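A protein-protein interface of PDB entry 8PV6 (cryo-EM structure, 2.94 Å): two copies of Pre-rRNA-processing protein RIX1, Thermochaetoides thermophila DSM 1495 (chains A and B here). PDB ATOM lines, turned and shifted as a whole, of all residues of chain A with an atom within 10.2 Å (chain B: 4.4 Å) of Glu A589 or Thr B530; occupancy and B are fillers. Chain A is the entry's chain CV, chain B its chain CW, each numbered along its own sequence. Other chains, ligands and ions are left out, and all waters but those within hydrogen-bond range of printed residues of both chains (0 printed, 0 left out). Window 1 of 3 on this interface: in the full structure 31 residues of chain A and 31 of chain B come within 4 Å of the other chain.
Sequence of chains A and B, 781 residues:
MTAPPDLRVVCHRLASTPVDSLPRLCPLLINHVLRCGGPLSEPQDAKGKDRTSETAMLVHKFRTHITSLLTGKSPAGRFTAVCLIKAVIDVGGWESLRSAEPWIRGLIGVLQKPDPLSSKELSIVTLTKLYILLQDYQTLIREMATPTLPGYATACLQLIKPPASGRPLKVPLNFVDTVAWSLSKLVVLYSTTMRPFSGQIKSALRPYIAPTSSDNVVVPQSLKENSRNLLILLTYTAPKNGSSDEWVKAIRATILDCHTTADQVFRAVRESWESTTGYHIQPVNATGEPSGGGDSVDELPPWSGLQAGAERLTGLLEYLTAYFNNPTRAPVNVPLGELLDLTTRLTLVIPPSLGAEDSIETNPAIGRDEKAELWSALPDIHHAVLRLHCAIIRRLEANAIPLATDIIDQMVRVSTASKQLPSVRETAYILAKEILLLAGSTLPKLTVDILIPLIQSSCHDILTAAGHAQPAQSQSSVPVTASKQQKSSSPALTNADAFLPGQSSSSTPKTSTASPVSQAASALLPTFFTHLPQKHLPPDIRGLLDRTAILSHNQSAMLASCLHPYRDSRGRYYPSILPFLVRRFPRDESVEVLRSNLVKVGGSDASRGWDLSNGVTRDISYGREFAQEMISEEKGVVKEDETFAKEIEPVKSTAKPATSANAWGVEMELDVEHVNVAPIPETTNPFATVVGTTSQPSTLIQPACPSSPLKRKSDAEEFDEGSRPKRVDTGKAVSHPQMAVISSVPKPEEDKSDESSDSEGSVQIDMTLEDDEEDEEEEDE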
ATOM      1  N   GLN A 555       2.223 -30.471  23.873  1.00  0.00           N
ATOM      2  CA  GLN A 555       3.578 -30.431  23.333  1.00  0.00           C
ATOM      3  C   GLN A 555       4.052 -31.808  22.873  1.00  0.00           C
ATOM      4  O   GLN A 555       4.679 -31.934  21.809  1.00  0.00           O
ATOM      5  CB  GLN A 555       4.482 -29.799  24.396  1.00  0.00           C
ATOM      6  CG  GLN A 555       4.646 -30.593  25.681  1.00  0.00           C
ATOM      7  CD  GLN A 555       5.441 -29.848  26.725  1.00  0.00           C
ATOM      8  OE1 GLN A 555       6.458 -29.239  26.427  1.00  0.00           O
ATOM      9  NE2 GLN A 555       4.972 -29.895  27.966  1.00  0.00           N
ATOM     10  N   SER A 556       3.714 -32.856  23.628  1.00  0.00           N
ATOM     11  CA  SER A 556       4.046 -34.213  23.217  1.00  0.00           C
ATOM     12  C   SER A 556       3.279 -34.602  21.962  1.00  0.00           C
ATOM     13  O   SER A 556       3.818 -35.275  21.078  1.00  0.00           O
ATOM     14  CB  SER A 556       3.753 -35.188  24.354  1.00  0.00           C
ATOM     15  OG  SER A 556       4.552 -34.898  25.486  1.00  0.00           O
ATOM     16  N   LEU A 559       4.943 -32.784  18.950  1.00  0.00           N
ATOM     17  CA  LEU A 559       6.174 -33.473  18.562  1.00  0.00           C
ATOM     18  C   LEU A 559       5.894 -34.828  17.918  1.00  0.00           C
ATOM     19  O   LEU A 559       6.575 -35.204  16.954  1.00  0.00           O
ATOM     20  CB  LEU A 559       7.113 -33.612  19.763  1.00  0.00           C
ATOM     21  CG  LEU A 559       8.458 -34.306  19.521  1.00  0.00           C
ATOM     22  CD1 LEU A 559       9.551 -33.649  20.286  1.00  0.00           C
ATOM     23  CD2 LEU A 559       8.376 -35.731  20.021  1.00  0.00           C
ATOM     24  N   LEU A 563       6.991 -36.003  14.163  1.00  0.00           N
ATOM     25  CA  LEU A 563       7.834 -37.168  13.937  1.00  0.00           C
ATOM     26  C   LEU A 563       7.099 -38.341  13.302  1.00  0.00           C
ATOM     27  O   LEU A 563       7.747 -39.314  12.904  1.00  0.00           O
ATOM     28  CB  LEU A 563       8.474 -37.612  15.252  1.00  0.00           C
ATOM     29  CG  LEU A 563       9.432 -36.586  15.853  1.00  0.00           C
ATOM     30  CD1 LEU A 563      10.085 -37.153  17.083  1.00  0.00           C
ATOM     31  CD2 LEU A 563      10.480 -36.175  14.833  1.00  0.00           C
ATOM     32  N   LEU A 578       5.618 -28.167  13.386  1.00  0.00           N
ATOM     33  CA  LEU A 578       6.824 -27.596  13.994  1.00  0.00           C
ATOM     34  C   LEU A 578       6.906 -26.067  14.093  1.00  0.00           C
ATOM     35  O   LEU A 578       7.414 -25.575  15.111  1.00  0.00           O
ATOM     36  CB  LEU A 578       8.061 -28.128  13.259  1.00  0.00           C
ATOM     37  CG  LEU A 578       9.404 -27.905  13.951  1.00  0.00           C
ATOM     38  CD1 LEU A 578       9.366 -28.447  15.365  1.00  0.00           C
ATOM     39  CD2 LEU A 578      10.525 -28.542  13.158  1.00  0.00           C
ATOM     40  N   LEU A 581       4.997 -25.571  17.182  1.00  0.00           N
ATOM     41  CA  LEU A 581       5.696 -26.103  18.346  1.00  0.00           C
ATOM     42  C   LEU A 581       6.806 -25.173  18.819  1.00  0.00           C
ATOM     43  O   LEU A 581       6.962 -24.962  20.026  1.00  0.00           O
ATOM     44  CB  LEU A 581       6.270 -27.484  18.030  1.00  0.00           C
ATOM     45  CG  LEU A 581       6.850 -28.296  19.193  1.00  0.00           C
ATOM     46  CD1 LEU A 581       5.960 -28.236  20.417  1.00  0.00           C
ATOM     47  CD2 LEU A 581       7.082 -29.733  18.775  1.00  0.00           C
ATOM     48  N   PHE A 585       6.465 -23.551  22.503  1.00  0.00           N
ATOM     49  CA  PHE A 585       7.457 -24.055  23.454  1.00  0.00           C
ATOM     50  C   PHE A 585       8.832 -23.920  22.819  1.00  0.00           C
ATOM     51  O   PHE A 585       9.357 -24.878  22.235  1.00  0.00           O
ATOM     52  CB  PHE A 585       7.163 -25.503  23.846  1.00  0.00           C
ATOM     53  CG  PHE A 585       5.759 -25.725  24.324  1.00  0.00           C
ATOM     54  CD1 PHE A 585       5.393 -25.394  25.617  1.00  0.00           C
ATOM     55  CD2 PHE A 585       4.802 -26.256  23.477  1.00  0.00           C
ATOM     56  CE1 PHE A 585       4.102 -25.595  26.059  1.00  0.00           C
ATOM     57  CE2 PHE A 585       3.508 -26.454  23.913  1.00  0.00           C
ATOM     58  CZ  PHE A 585       3.160 -26.127  25.206  1.00  0.00           C
ATOM     59  N   PRO A 586       9.447 -22.740  22.911  1.00  0.00           N
ATOM     60  CA  PRO A 586      10.688 -22.491  22.166  1.00  0.00           C
ATOM     61  C   PRO A 586      11.936 -23.082  22.797  1.00  0.00           C
ATOM     62  O   PRO A 586      12.930 -23.311  22.103  1.00  0.00           O
ATOM     63  CB  PRO A 586      10.764 -20.962  22.136  1.00  0.00           C
ATOM     64  CG  PRO A 586      10.061 -20.539  23.371  1.00  0.00           C
ATOM     65  CD  PRO A 586       8.964 -21.534  23.606  1.00  0.00           C
ATOM     66  N   ARG A 587      11.910 -23.326  24.101  1.00  0.00           N
ATOM     67  CA  ARG A 587      13.097 -23.731  24.841  1.00  0.00           C
ATOM     68  C   ARG A 587      12.831 -24.985  25.662  1.00  0.00           C
ATOM     69  O   ARG A 587      13.425 -25.204  26.719  1.00  0.00           O
ATOM     70  CB  ARG A 587      13.592 -22.580  25.709  1.00  0.00           C
ATOM     71  CG  ARG A 587      12.578 -22.074  26.720  1.00  0.00           C
ATOM     72  CD  ARG A 587      13.002 -20.731  27.279  1.00  0.00           C
ATOM     73  NE  ARG A 587      12.924 -19.692  26.259  1.00  0.00           N
ATOM     74  CZ  ARG A 587      13.973 -19.124  25.682  1.00  0.00           C
ATOM     75  NH1 ARG A 587      15.209 -19.460  26.011  1.00  0.00           N
ATOM     76  NH2 ARG A 587      13.776 -18.200  24.746  1.00  0.00           N
ATOM     77  N   ASP A 588      11.940 -25.831  25.164  1.00  0.00           N
ATOM     78  CA  ASP A 588      11.632 -27.111  25.776  1.00  0.00           C
ATOM     79  C   ASP A 588      12.608 -28.170  25.269  1.00  0.00           C
ATOM     80  O   ASP A 588      13.251 -28.007  24.230  1.00  0.00           O
ATOM     81  CB  ASP A 588      10.188 -27.516  25.456  1.00  0.00           C
ATOM     82  CG  ASP A 588       9.752 -28.766  26.187  1.00  0.00           C
ATOM     83  OD1 ASP A 588      10.194 -28.970  27.337  1.00  0.00           O
ATOM     84  OD2 ASP A 588       9.030 -29.581  25.586  1.00  0.00           O
ATOM     85  N   GLU A 589      12.711 -29.267  26.029  1.00  0.00           N
ATOM     86  CA  GLU A 589      13.492 -30.426  25.605  1.00  0.00           C
ATOM     87  C   GLU A 589      12.988 -30.986  24.276  1.00  0.00           C
ATOM     88  O   GLU A 589      13.772 -31.527  23.485  1.00  0.00           O
ATOM     89  CB  GLU A 589      13.433 -31.499  26.693  1.00  0.00           C
ATOM     90  CG  GLU A 589      14.448 -32.617  26.567  1.00  0.00           C
ATOM     91  CD  GLU A 589      15.850 -32.178  26.934  1.00  0.00           C
ATOM     92  OE1 GLU A 589      15.990 -31.187  27.682  1.00  0.00           O
ATOM     93  OE2 GLU A 589      16.812 -32.834  26.489  1.00  0.00           O
ATOM     94  N   SER A 590      11.687 -30.832  24.008  1.00  0.00           N
ATOM     95  CA  SER A 590      11.079 -31.343  22.782  1.00  0.00           C
ATOM     96  C   SER A 590      11.674 -30.694  21.537  1.00  0.00           C
ATOM     97  O   SER A 590      11.886 -31.358  20.517  1.00  0.00           O
ATOM     98  CB  SER A 590       9.569 -31.115  22.827  1.00  0.00           C
ATOM     99  OG  SER A 590       9.017 -31.600  24.037  1.00  0.00           O
ATOM    100  N   VAL A 591      11.937 -29.390  21.592  1.00  0.00           N
ATOM    101  CA  VAL A 591      12.555 -28.741  20.441  1.00  0.00           C
ATOM    102  C   VAL A 591      14.076 -28.745  20.560  1.00  0.00           C
ATOM    103  O   VAL A 591      14.783 -28.665  19.543  1.00  0.00           O
ATOM    104  CB  VAL A 591      11.993 -27.321  20.265  1.00  0.00           C
ATOM    105  CG1 VAL A 591      10.514 -27.386  19.941  1.00  0.00           C
ATOM    106  CG2 VAL A 591      12.207 -26.508  21.518  1.00  0.00           C
ATOM    107  N   GLU A 592      14.612 -28.859  21.779  1.00  0.00           N
ATOM    108  CA  GLU A 592      16.055 -28.997  21.931  1.00  0.00           C
ATOM    109  C   GLU A 592      16.583 -30.315  21.382  1.00  0.00           C
ATOM    110  O   GLU A 592      17.754 -30.372  20.996  1.00  0.00           O
ATOM    111  CB  GLU A 592      16.460 -28.852  23.398  1.00  0.00           C
ATOM    112  CG  GLU A 592      16.387 -27.428  23.932  1.00  0.00           C
ATOM    113  CD  GLU A 592      17.384 -26.498  23.274  1.00  0.00           C
ATOM    114  OE1 GLU A 592      18.496 -26.955  22.933  1.00  0.00           O
ATOM    115  OE2 GLU A 592      17.055 -25.307  23.096  1.00  0.00           O
ATOM    116  N   VAL A 593      15.764 -31.365  21.335  1.00  0.00           N
ATOM    117  CA  VAL A 593      16.192 -32.595  20.675  1.00  0.00           C
ATOM    118  C   VAL A 593      16.012 -32.538  19.161  1.00  0.00           C
ATOM    119  O   VAL A 593      16.741 -33.235  18.441  1.00  0.00           O
ATOM    120  CB  VAL A 593      15.482 -33.840  21.250  1.00  0.00           C
ATOM    121  CG1 VAL A 593      15.792 -33.982  22.719  1.00  0.00           C
ATOM    122  CG2 VAL A 593      13.985 -33.780  21.024  1.00  0.00           C
ATOM    123  N   LEU A 594      15.083 -31.729  18.655  1.00  0.00           N
ATOM    124  CA  LEU A 594      14.972 -31.527  17.217  1.00  0.00           C
ATOM    125  C   LEU A 594      16.031 -30.577  16.680  1.00  0.00           C
ATOM    126  O   LEU A 594      16.283 -30.575  15.471  1.00  0.00           O
ATOM    127  CB  LEU A 594      13.577 -31.012  16.858  1.00  0.00           C
ATOM    128  CG  LEU A 594      12.505 -32.095  16.746  1.00  0.00           C
ATOM    129  CD1 LEU A 594      11.137 -31.481  16.542  1.00  0.00           C
ATOM    130  CD2 LEU A 594      12.838 -33.056  15.617  1.00  0.00           C
ATOM    131  N   ARG A 595      16.648 -29.775  17.544  1.00  0.00           N
ATOM    132  CA  ARG A 595      17.788 -28.951  17.164  1.00  0.00           C
ATOM    133  C   ARG A 595      19.120 -29.674  17.332  1.00  0.00           C
ATOM    134  O   ARG A 595      20.143 -29.021  17.554  1.00  0.00           O
ATOM    135  CB  ARG A 595      17.802 -27.654  17.971  1.00  0.00           C
ATOM    136  CG  ARG A 595      16.752 -26.657  17.543  1.00  0.00           C
ATOM    137  CD  ARG A 595      17.001 -25.308  18.179  1.00  0.00           C
ATOM    138  NE  ARG A 595      16.245 -25.134  19.411  1.00  0.00           N
ATOM    139  CZ  ARG A 595      15.156 -24.386  19.515  1.00  0.00           C
ATOM    140  NH1 ARG A 595      14.650 -23.753  18.470  1.00  0.00           N
ATOM    141  NH2 ARG A 595      14.563 -24.266  20.697  1.00  0.00           N
ATOM    142  N   SER A 596      19.131 -31.005  17.230  1.00  0.00           N
ATOM    143  CA  SER A 596      20.350 -31.767  17.475  1.00  0.00           C
ATOM    144  C   SER A 596      21.297 -31.769  16.283  1.00  0.00           C
ATOM    145  O   SER A 596      22.413 -32.284  16.399  1.00  0.00           O
ATOM    146  CB  SER A 596      20.000 -33.204  17.849  1.00  0.00           C
ATOM    147  OG  SER A 596      19.059 -33.229  18.905  1.00  0.00           O
ATOM    148  N   VAL A 599      24.697 -29.696  16.939  1.00  0.00           N
ATOM    149  CA  VAL A 599      25.458 -29.980  18.153  1.00  0.00           C
ATOM    150  C   VAL A 599      26.958 -29.838  17.919  1.00  0.00           C
ATOM    151  O   VAL A 599      27.663 -29.240  18.746  1.00  0.00           O
ATOM    152  CB  VAL A 599      25.080 -31.377  18.681  1.00  0.00           C
ATOM    153  CG1 VAL A 599      26.115 -31.898  19.664  1.00  0.00           C
ATOM    154  CG2 VAL A 599      23.714 -31.321  19.339  1.00  0.00           C
ATOM    155  N   PRO B 526      18.603 -33.115  35.287  1.00  0.00           N
ATOM    156  CA  PRO B 526      18.799 -32.623  33.908  1.00  0.00           C
ATOM    157  C   PRO B 526      19.150 -31.148  33.822  1.00  0.00           C
ATOM    158  O   PRO B 526      19.687 -30.703  32.796  1.00  0.00           O
ATOM    159  CB  PRO B 526      17.448 -32.912  33.239  1.00  0.00           C
ATOM    160  CG  PRO B 526      16.851 -33.978  34.052  1.00  0.00           C
ATOM    161  CD  PRO B 526      17.226 -33.621  35.443  1.00  0.00           C
ATOM    162  N   THR B 527      18.856 -30.374  34.868  1.00  0.00           N
ATOM    163  CA  THR B 527      19.177 -28.953  34.855  1.00  0.00           C
ATOM    164  C   THR B 527      20.683 -28.730  34.938  1.00  0.00           C
ATOM    165  O   THR B 527      21.197 -27.722  34.439  1.00  0.00           O
ATOM    166  CB  THR B 527      18.453 -28.247  36.001  1.00  0.00           C
ATOM    167  OG1 THR B 527      17.101 -28.714  36.060  1.00  0.00           O
ATOM    168  CG2 THR B 527      18.423 -26.755  35.773  1.00  0.00           C
ATOM    169  N   PHE B 528      21.413 -29.681  35.531  1.00  0.00           N
ATOM    170  CA  PHE B 528      22.867 -29.568  35.598  1.00  0.00           C
ATOM    171  C   PHE B 528      23.500 -29.677  34.217  1.00  0.00           C
ATOM    172  O   PHE B 528      24.603 -29.169  33.991  1.00  0.00           O
ATOM    173  CB  PHE B 528      23.441 -30.637  36.526  1.00  0.00           C
ATOM    174  CG  PHE B 528      23.114 -30.423  37.972  1.00  0.00           C
ATOM    175  CD1 PHE B 528      23.133 -29.153  38.516  1.00  0.00           C
ATOM    176  CD2 PHE B 528      22.821 -31.495  38.795  1.00  0.00           C
ATOM    177  CE1 PHE B 528      22.841 -28.953  39.846  1.00  0.00           C
ATOM    178  CE2 PHE B 528      22.532 -31.301  40.126  1.00  0.00           C
ATOM    179  CZ  PHE B 528      22.546 -30.027  40.652  1.00  0.00           C
ATOM    180  N   PHE B 529      22.822 -30.346  33.283  1.00  0.00           N
ATOM    181  CA  PHE B 529      23.317 -30.391  31.912  1.00  0.00           C
ATOM    182  C   PHE B 529      22.767 -29.231  31.092  1.00  0.00           C
ATOM    183  O   PHE B 529      23.503 -28.585  30.340  1.00  0.00           O
ATOM    184  CB  PHE B 529      22.952 -31.720  31.251  1.00  0.00           C
ATOM    185  CG  PHE B 529      23.316 -32.932  32.055  1.00  0.00           C
ATOM    186  CD1 PHE B 529      22.390 -33.530  32.890  1.00  0.00           C
ATOM    187  CD2 PHE B 529      24.577 -33.490  31.956  1.00  0.00           C
ATOM    188  CE1 PHE B 529      22.718 -34.651  33.620  1.00  0.00           C
ATOM    189  CE2 PHE B 529      24.910 -34.611  32.683  1.00  0.00           C
ATOM    190  CZ  PHE B 529      23.980 -35.191  33.516  1.00  0.00           C
ATOM    191  N   THR B 530      21.463 -28.962  31.214  1.00  0.00           N
ATOM    192  CA  THR B 530      20.837 -27.982  30.329  1.00  0.00           C
ATOM    193  C   THR B 530      21.216 -26.553  30.696  1.00  0.00           C
ATOM    194  O   THR B 530      21.539 -25.748  29.815  1.00  0.00           O
ATOM    195  CB  THR B 530      19.318 -28.136  30.345  1.00  0.00           C
ATOM    196  OG1 THR B 530      18.848 -28.146  31.698  1.00  0.00           O
ATOM    197  CG2 THR B 530      18.901 -29.417  29.657  1.00  0.00           C
ATOM    198  N   HIS B 531      21.185 -26.214  31.983  1.00  0.00           N
ATOM    199  CA  HIS B 531      21.302 -24.829  32.417  1.00  0.00           C
ATOM    200  C   HIS B 531      22.511 -24.582  33.307  1.00  0.00           C
ATOM    201  O   HIS B 531      22.392 -23.879  34.316  1.00  0.00           O
ATOM    202  CB  HIS B 531      20.027 -24.403  33.140  1.00  0.00           C
ATOM    203  CG  HIS B 531      18.858 -24.200  32.229  1.00  0.00           C
ATOM    204  ND1 HIS B 531      17.977 -25.211  31.915  1.00  0.00           N
ATOM    205  CD2 HIS B 531      18.429 -23.105  31.560  1.00  0.00           C
ATOM    206  CE1 HIS B 531      17.053 -24.747  31.094  1.00  0.00           C
ATOM    207  NE2 HIS B 531      17.304 -23.471  30.862  1.00  0.00           N
ATOM    208  N   LEU B 532      23.664 -25.143  32.968  1.00  0.00           N
ATOM    209  CA  LEU B 532      24.899 -24.860  33.669  1.00  0.00           C
ATOM    210  C   LEU B 532      26.026 -24.745  32.654  1.00  0.00           C
ATOM    211  O   LEU B 532      26.005 -25.451  31.635  1.00  0.00           O
ATOM    212  CB  LEU B 532      25.212 -25.964  34.690  1.00  0.00           C
ATOM    213  CG  LEU B 532      25.877 -25.556  36.005  1.00  0.00           C
ATOM    214  CD1 LEU B 532      25.096 -24.441  36.669  1.00  0.00           C
ATOM    215  CD2 LEU B 532      25.989 -26.749  36.933  1.00  0.00           C
ATOM    216  N   LEU B 559      19.399 -37.661  28.048  1.00  0.00           N
ATOM    217  CA  LEU B 559      19.120 -36.922  26.826  1.00  0.00           C
ATOM    218  C   LEU B 559      19.802 -35.560  26.843  1.00  0.00           C
ATOM    219  O   LEU B 559      20.406 -35.142  25.847  1.00  0.00           O
ATOM    220  CB  LEU B 559      17.604 -36.776  26.692  1.00  0.00           C
ATOM    221  CG  LEU B 559      16.855 -36.613  25.378  1.00  0.00           C
ATOM    222  CD1 LEU B 559      16.763 -37.948  24.683  1.00  0.00           C
ATOM    223  CD2 LEU B 559      15.466 -36.104  25.692  1.00  0.00           C
ATOM    224  N   ALA B 560      19.741 -34.868  27.985  1.00  0.00           N
ATOM    225  CA  ALA B 560      20.411 -33.581  28.127  1.00  0.00           C
ATOM    226  C   ALA B 560      21.926 -33.730  28.070  1.00  0.00           C
ATOM    227  O   ALA B 560      22.621 -32.871  27.514  1.00  0.00           O
ATOM    228  CB  ALA B 560      19.985 -32.924  29.435  1.00  0.00           C
ATOM    229  N   LEU B 563      22.824 -34.097  24.560  1.00  0.00           N
ATOM    230  CA  LEU B 563      22.664 -32.834  23.844  1.00  0.00           C
ATOM    231  C   LEU B 563      23.791 -31.858  24.159  1.00  0.00           C
ATOM    232  O   LEU B 563      24.159 -31.036  23.314  1.00  0.00           O
ATOM    233  CB  LEU B 563      21.314 -32.207  24.176  1.00  0.00           C
ATOM    234  CG  LEU B 563      20.119 -32.781  23.423  1.00  0.00           C
ATOM    235  CD1 LEU B 563      18.836 -32.221  23.985  1.00  0.00           C
ATOM    236  CD2 LEU B 563      20.242 -32.450  21.951  1.00  0.00           C
ATOM    237  N   HIS B 564      24.339 -31.919  25.370  1.00  0.00           N
ATOM    238  CA  HIS B 564      25.415 -31.013  25.760  1.00  0.00           C
ATOM    239  C   HIS B 564      26.719 -31.781  25.920  1.00  0.00           C
ATOM    240  O   HIS B 564      26.943 -32.396  26.974  1.00  0.00           O
ATOM    241  CB  HIS B 564      25.068 -30.290  27.061  1.00  0.00           C
ATOM    242  CG  HIS B 564      23.813 -29.481  26.988  1.00  0.00           C
ATOM    243  ND1 HIS B 564      22.557 -30.046  27.047  1.00  0.00           N
ATOM    244  CD2 HIS B 564      23.619 -28.147  26.869  1.00  0.00           C
ATOM    245  CE1 HIS B 564      21.644 -29.095  26.962  1.00  0.00           C
ATOM    246  NE2 HIS B 564      22.262 -27.933  26.853  1.00  0.00           N
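2 positions are printed for both chains. Of the 8 pairs that touch across the chains among the printed residues, none has its exchanged pair printed and touching as well.
The side-chain hydroxyl (OG1) of Thr B530 lies within hydrogen-bond range of the backbone carbonyl oxygen (O) of Pro B526, at 2.9 Å. OG1 of Thr B530 is in hydrogen-bond range of ND1 of His B531 (3.1 Å). The guanidinium group (NH2) of Arg A595 lies within salt-bridge range of the side-chain carboxylate (OE2) of Glu A592 (3.6 Å). The backbone carbonyl oxygen of Ala B560 sits at hydrogen-bond distance from a ring nitrogen (ND1) of His B564 (2.9 Å).
Gln A555 touches none of the printed residues of chain B. Of chain B, only Thr B530 (3.9 Å), Leu B559 (3.6 Å), Ala B560 (3.9 Å) and Leu B563 (3.3 Å) come within 4 Å of Glu A589. Val A591 touches none of the printed residues of chain B. Printed residues of chain B within 4 Å of Glu A592: Leu B563. Of the printed residues of chain B, Val A593 touches Leu B559 (3.7 Å) and Leu B563 (3.7 Å). Of the printed residues of chain B, Ser A596 touches Leu B563. No residue of chain A comes within 4 Å of Thr B527. No residue of chain A comes within 4 Å of His B531. Leu B559 touches just these residues of chain A: Glu A589 and Val A593. Of the printed residues of chain A, Leu B563 touches Glu A589, Glu A592, Val A593 and Ser A596. The nearest residue of chain A that does not touch Thr B530 is Glu A592 (6.6 Å).
Hydrophobic or aromatic side chains of chain A that line the printed part of chain B: Val A593. Of the 11 printed residues of chain B, 4 touch a printed residue of chain A. Hydrophobic or aromatic side chains of chain B that line the printed part of chain A: Leu B559 and Leu B563. Among the printed residues, 8 pairs touch across the chains. Among the printed residues, no Asp or Glu carboxylate lies within 4 Å of a Lys or Arg side-chain nitrogen of the other chain.
Among the printed residues, merely in contact across the chains: Glu A589 with Leu B563, Ser A596 with Leu B563, Glu A592 with Leu B563, Glu A589 with Leu B559, Val A593 with Leu B559, Val A593 with Leu B563, Glu A589 with Ala B560 and Glu A589 with Thr B530.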
